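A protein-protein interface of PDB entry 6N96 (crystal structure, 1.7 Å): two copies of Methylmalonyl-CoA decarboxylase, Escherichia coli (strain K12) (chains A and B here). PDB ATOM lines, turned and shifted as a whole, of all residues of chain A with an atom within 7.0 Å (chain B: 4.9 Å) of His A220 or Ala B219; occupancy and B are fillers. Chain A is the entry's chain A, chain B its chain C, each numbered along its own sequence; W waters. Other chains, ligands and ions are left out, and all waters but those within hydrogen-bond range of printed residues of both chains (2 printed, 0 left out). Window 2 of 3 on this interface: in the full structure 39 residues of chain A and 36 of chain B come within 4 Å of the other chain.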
ATOM      1  N   HIS A 146      -7.385 -10.917  30.422  1.00  0.00           N
ATOM      2  CA  HIS A 146      -6.523 -10.674  29.236  1.00  0.00           C
ATOM      3  C   HIS A 146      -6.129 -12.026  28.634  1.00  0.00           C
ATOM      4  O   HIS A 146      -6.112 -12.158  27.408  1.00  0.00           O
ATOM      5  CB  HIS A 146      -5.278  -9.883  29.665  1.00  0.00           C
ATOM      6  CG  HIS A 146      -4.646  -9.064  28.594  1.00  0.00           C
ATOM      7  ND1 HIS A 146      -4.959  -9.210  27.259  1.00  0.00           N
ATOM      8  CD2 HIS A 146      -3.678  -8.126  28.662  1.00  0.00           C
ATOM      9  CE1 HIS A 146      -4.224  -8.371  26.543  1.00  0.00           C
ATOM     10  NE2 HIS A 146      -3.451  -7.675  27.392  1.00  0.00           N
ATOM     11  N   THR A 149      -8.453 -13.577  25.956  1.00  0.00           N
ATOM     12  CA  THR A 149      -8.879 -12.746  24.816  1.00  0.00           C
ATOM     13  C   THR A 149      -7.981 -12.922  23.587  1.00  0.00           C
ATOM     14  O   THR A 149      -8.197 -12.189  22.614  1.00  0.00           O
ATOM     15  CB  THR A 149      -8.881 -11.241  25.175  1.00  0.00           C
ATOM     16  OG1 THR A 149      -7.556 -10.772  25.409  1.00  0.00           O
ATOM     17  CG2 THR A 149      -9.782 -10.940  26.344  1.00  0.00           C
ATOM     18  N   ARG A 150      -7.022 -13.839  23.601  1.00  0.00           N
ATOM     19  CA  ARG A 150      -6.012 -13.901  22.502  1.00  0.00           C
ATOM     20  C   ARG A 150      -6.368 -14.982  21.479  1.00  0.00           C
ATOM     21  O   ARG A 150      -5.583 -15.143  20.511  1.00  0.00           O
ATOM     22  CB  ARG A 150      -4.599 -14.132  23.060  1.00  0.00           C
ATOM     23  CG  ARG A 150      -4.224 -13.109  24.108  1.00  0.00           C
ATOM     24  CD  ARG A 150      -2.727 -13.093  24.363  1.00  0.00           C
ATOM     25  NE  ARG A 150      -2.434 -12.026  25.315  1.00  0.00           N
ATOM     26  CZ  ARG A 150      -2.415 -12.179  26.638  1.00  0.00           C
ATOM     27  NH1 ARG A 150      -2.462 -13.378  27.189  1.00  0.00           N
ATOM     28  NH2 ARG A 150      -2.204 -11.130  27.412  1.00  0.00           N
ATOM     29  N   VAL A 215       5.292 -10.941  25.262  1.00  0.00           N
ATOM     30  CA  VAL A 215       5.342  -9.471  25.523  1.00  0.00           C
ATOM     31  C   VAL A 215       4.416  -8.735  24.553  1.00  0.00           C
ATOM     32  O   VAL A 215       3.739  -7.790  25.033  1.00  0.00           O
ATOM     33  CB  VAL A 215       6.766  -8.887  25.592  1.00  0.00           C
ATOM     34  CG1 VAL A 215       7.499  -9.452  26.801  1.00  0.00           C
ATOM     35  CG2 VAL A 215       7.585  -9.101  24.325  1.00  0.00           C
ATOM     36  N   LEU A 216       4.286  -9.163  23.303  1.00  0.00           N
ATOM     37  CA  LEU A 216       3.299  -8.521  22.412  1.00  0.00           C
ATOM     38  C   LEU A 216       1.892  -8.744  22.949  1.00  0.00           C
ATOM     39  O   LEU A 216       1.049  -7.815  22.869  1.00  0.00           O
ATOM     40  CB  LEU A 216       3.434  -9.048  20.975  1.00  0.00           C
ATOM     41  CG  LEU A 216       4.686  -8.591  20.234  1.00  0.00           C
ATOM     42  CD1 LEU A 216       4.893  -9.471  18.995  1.00  0.00           C
ATOM     43  CD2 LEU A 216       4.617  -7.114  19.821  1.00  0.00           C
ATOM     44  N   GLY A 217       1.591  -9.938  23.454  1.00  0.00           N
ATOM     45  CA  GLY A 217       0.265 -10.221  24.022  1.00  0.00           C
ATOM     46  C   GLY A 217      -0.062  -9.404  25.249  1.00  0.00           C
ATOM     47  O   GLY A 217      -1.232  -9.095  25.432  1.00  0.00           O
ATOM     48  N   GLU A 218       0.926  -9.065  26.034  1.00  0.00           N
ATOM     49  CA  GLU A 218       0.742  -8.282  27.266  1.00  0.00           C
ATOM     50  C   GLU A 218       0.686  -6.793  26.974  1.00  0.00           C
ATOM     51  O   GLU A 218       0.106  -6.078  27.832  1.00  0.00           O
ATOM     52  CB  GLU A 218       1.828  -8.648  28.259  1.00  0.00           C
ATOM     53  CG  GLU A 218       1.484  -9.985  28.902  1.00  0.00           C
ATOM     54  CD  GLU A 218       2.256 -10.267  30.174  1.00  0.00           C
ATOM     55  OE1 GLU A 218       2.500  -9.260  30.888  1.00  0.00           O
ATOM     56  OE2 GLU A 218       2.679 -11.465  30.397  1.00  0.00           O
ATOM     57  N   ALA A 219       1.169  -6.360  25.803  1.00  0.00           N
ATOM     58  CA  ALA A 219       1.436  -4.926  25.497  1.00  0.00           C
ATOM     59  C   ALA A 219       0.139  -4.163  25.190  1.00  0.00           C
ATOM     60  O   ALA A 219       0.130  -3.371  24.228  1.00  0.00           O
ATOM     61  CB  ALA A 219       2.396  -4.861  24.354  1.00  0.00           C
ATOM     62  N   HIS A 220      -0.917  -4.353  25.995  1.00  0.00           N
ATOM     63  CA  HIS A 220      -2.080  -3.444  26.045  1.00  0.00           C
ATOM     64  C   HIS A 220      -1.896  -2.557  27.270  1.00  0.00           C
ATOM     65  O   HIS A 220      -1.946  -3.114  28.354  1.00  0.00           O
ATOM     66  CB  HIS A 220      -3.382  -4.231  26.144  1.00  0.00           C
ATOM     67  CG  HIS A 220      -3.731  -5.033  24.924  1.00  0.00           C
ATOM     68  ND1 HIS A 220      -2.813  -5.841  24.279  1.00  0.00           N
ATOM     69  CD2 HIS A 220      -4.923  -5.242  24.305  1.00  0.00           C
ATOM     70  CE1 HIS A 220      -3.391  -6.446  23.257  1.00  0.00           C
ATOM     71  NE2 HIS A 220      -4.683  -6.075  23.231  1.00  0.00           N
ATOM     72  N   THR A 221      -1.583  -1.284  27.123  1.00  0.00           N
ATOM     73  CA  THR A 221      -1.099  -0.463  28.250  1.00  0.00           C
ATOM     74  C   THR A 221      -2.185   0.536  28.617  1.00  0.00           C
ATOM     75  O   THR A 221      -3.016   0.925  27.756  1.00  0.00           O
ATOM     76  CB  THR A 221       0.260   0.183  27.981  1.00  0.00           C
ATOM     77  OG1 THR A 221       0.153   1.103  26.896  1.00  0.00           O
ATOM     78  CG2 THR A 221       1.334  -0.857  27.726  1.00  0.00           C
ATOM     79  N   MET A 222      -2.217   0.892  29.896  1.00  0.00           N
ATOM     80  CA  MET A 222      -3.182   1.868  30.437  1.00  0.00           C
ATOM     81  C   MET A 222      -2.450   2.698  31.487  1.00  0.00           C
ATOM     82  O   MET A 222      -1.339   2.307  31.879  1.00  0.00           O
ATOM     83  CB  MET A 222      -4.415   1.184  31.055  1.00  0.00           C
ATOM     84  CG  MET A 222      -4.097   0.317  32.241  1.00  0.00           C
ATOM     85  SD  MET A 222      -5.542  -0.641  32.821  1.00  0.00           S
ATOM     86  CE  MET A 222      -5.957  -1.390  31.236  1.00  0.00           C
ATOM     87  N   VAL B 215     -11.806  -1.826  28.832  1.00  0.00           N
ATOM     88  CA  VAL B 215     -10.505  -1.124  29.018  1.00  0.00           C
ATOM     89  C   VAL B 215      -9.397  -1.867  28.255  1.00  0.00           C
ATOM     90  O   VAL B 215      -8.560  -1.182  27.584  1.00  0.00           O
ATOM     91  CB  VAL B 215     -10.233  -0.959  30.523  1.00  0.00           C
ATOM     92  CG1 VAL B 215      -8.806  -0.537  30.779  1.00  0.00           C
ATOM     93  CG2 VAL B 215     -11.204   0.037  31.124  1.00  0.00           C
ATOM     94  N   LEU B 216      -9.362  -3.194  28.362  1.00  0.00           N
ATOM     95  CA  LEU B 216      -8.328  -3.971  27.626  1.00  0.00           C
ATOM     96  C   LEU B 216      -8.520  -3.751  26.126  1.00  0.00           C
ATOM     97  O   LEU B 216      -7.524  -3.547  25.408  1.00  0.00           O
ATOM     98  CB  LEU B 216      -8.417  -5.461  28.012  1.00  0.00           C
ATOM     99  CG  LEU B 216      -7.902  -5.757  29.411  1.00  0.00           C
ATOM    100  CD1 LEU B 216      -8.308  -7.156  29.881  1.00  0.00           C
ATOM    101  CD2 LEU B 216      -6.371  -5.594  29.500  1.00  0.00           C
ATOM    102  N   GLY B 217      -9.764  -3.758  25.646  1.00  0.00           N
ATOM    103  CA  GLY B 217     -10.034  -3.580  24.217  1.00  0.00           C
ATOM    104  C   GLY B 217      -9.596  -2.228  23.710  1.00  0.00           C
ATOM    105  O   GLY B 217      -9.243  -2.154  22.524  1.00  0.00           O
ATOM    106  N   GLU B 218      -9.635  -1.215  24.552  1.00  0.00           N
ATOM    107  CA  GLU B 218      -9.287   0.175  24.162  1.00  0.00           C
ATOM    108  C   GLU B 218      -7.784   0.388  24.278  1.00  0.00           C
ATOM    109  O   GLU B 218      -7.301   1.384  23.700  1.00  0.00           O
ATOM    110  CB  GLU B 218     -10.049   1.190  25.021  1.00  0.00           C
ATOM    111  CG  GLU B 218     -11.535   1.174  24.691  1.00  0.00           C
ATOM    112  CD  GLU B 218     -12.278   2.464  25.036  1.00  0.00           C
ATOM    113  OE1 GLU B 218     -11.591   3.495  25.228  1.00  0.00           O
ATOM    114  OE2 GLU B 218     -13.564   2.429  25.140  1.00  0.00           O
ATOM    115  N   ALA B 219      -7.065  -0.487  24.977  1.00  0.00           N
ATOM    116  CA  ALA B 219      -5.676  -0.194  25.432  1.00  0.00           C
ATOM    117  C   ALA B 219      -4.645  -0.406  24.301  1.00  0.00           C
ATOM    118  O   ALA B 219      -3.653  -1.119  24.511  1.00  0.00           O
ATOM    119  CB  ALA B 219      -5.394  -1.013  26.655  1.00  0.00           C
ATOM    120  N   HIS B 220      -4.899   0.123  23.116  1.00  0.00           N
ATOM    121  CA  HIS B 220      -3.929   0.248  22.000  1.00  0.00           C
ATOM    122  C   HIS B 220      -3.557   1.726  21.967  1.00  0.00           C
ATOM    123  O   HIS B 220      -4.447   2.523  21.719  1.00  0.00           O
ATOM    124  CB  HIS B 220      -4.576  -0.119  20.653  1.00  0.00           C
ATOM    125  CG  HIS B 220      -4.935  -1.571  20.506  1.00  0.00           C
ATOM    126  ND1 HIS B 220      -4.722  -2.247  19.310  1.00  0.00           N
ATOM    127  CD2 HIS B 220      -5.631  -2.423  21.289  1.00  0.00           C
ATOM    128  CE1 HIS B 220      -5.127  -3.503  19.433  1.00  0.00           C
ATOM    129  NE2 HIS B 220      -5.710  -3.634  20.629  1.00  0.00           N
ATOM    130  N   THR B 221      -2.387   2.086  22.423  1.00  0.00           N
ATOM    131  CA  THR B 221      -2.102   3.507  22.728  1.00  0.00           C
ATOM    132  C   THR B 221      -1.101   3.995  21.695  1.00  0.00           C
ATOM    133  O   THR B 221      -0.285   3.186  21.167  1.00  0.00           O
ATOM    134  CB  THR B 221      -1.621   3.711  24.168  1.00  0.00           C
ATOM    135  OG1 THR B 221      -0.417   2.983  24.348  1.00  0.00           O
ATOM    136  CG2 THR B 221      -2.600   3.225  25.187  1.00  0.00           C
HETATM  137  O   HOH W   1      -4.952  -6.935  20.143  1.00  0.00           O
HETATM  138  O   HOH W   2      -0.612  -0.137  24.052  1.00  0.00           O
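The backbone carbonyl oxygen (O) of Ala B219 lies within hydrogen-bond range of the backbone NH (N) of Thr A221 (3.3 Å).
The side-chain hydroxyl (OG1) of Thr A221 sits at hydrogen-bond distance from the side-chain hydroxyl (OG1) of Thr B221 (3.2 Å).
Of the 7 printed residues of chain B, 5 touch a printed residue of chain A.
Printed residues of chain B that touch a printed residue of chain A: Val B215, Leu B216, Ala B219, His B220 and Thr B221.
Of the 11 printed residues of chain A, 4 touch a printed residue of chain B.
Printed residues of chain A that touch a printed residue of chain B: His A146, His A220, Thr A221 and Met A222.
Hydrophobic or aromatic side chains of chain A within 4 Å of the printed part of chain B: His A146, His A220 and Met A222.
Among the printed residues, 7 pairs touch across the chains.
Leu A216 touches none of the printed residues of chain B.
Ala A219 touches none of the printed residues of chain B.
Of the printed residues of chain B, Met A222 touches Val B215 (3.0 Å).
Of the printed residues of chain A, Val B215 touches Met A222.
Printed residues of chain A within 4 Å of Ala B219: His A220 (3.2 Å) and Thr A221 (3.3 Å).
The nearest printed residue of chain A that does not touch Thr B221 is Met A222 (5.3 Å).
Among the printed residues, merely in contact across the chains: His A146 with Leu B216, His A220 with Leu B216, His A220 with Ala B219, His A220 with His B220 and Met A222 with Val B215.
O of His A146 sits at hydrogen-bond distance from OG1 of Thr A149.
ND1 of His A146 sits at hydrogen-bond distance from NH2 of Arg A150, at 3.4 Å.
A ring nitrogen (NE2) of His A146 lies close to the backbone carbonyl oxygen (O) of Gly A217 (3.3 Å).
Water W2 lies within hydrogen-bond range of the side-chain hydroxyl (OG1) of Thr B221 (3.1 Å), the side-chain hydroxyl (OG1) of Thr A221 (3.2 Å), the backbone carbonyl oxygen (O) of Ala B219 (3.2 Å) and the backbone carbonyl oxygen (O) of Ala A219 (3.3 Å).
Water W1 lies within hydrogen-bond range of a ring nitrogen (NE2) of His A220 and a ring nitrogen (NE2) of His B220.
His A220 touches Leu B216, but with the chains exchanged Leu A216 does not touch His B220 (8.3 Å).
His A220 touches its own counterpart, His B220.
Thr A221 touches Ala B219, but with the chains exchanged Ala A219 does not touch Thr B221 (6.3 Å).
Thr B221 touches its own counterpart, Thr A221.
Positions printed for both chains: 215, 216, 217, 218, 219, 220 and 221.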
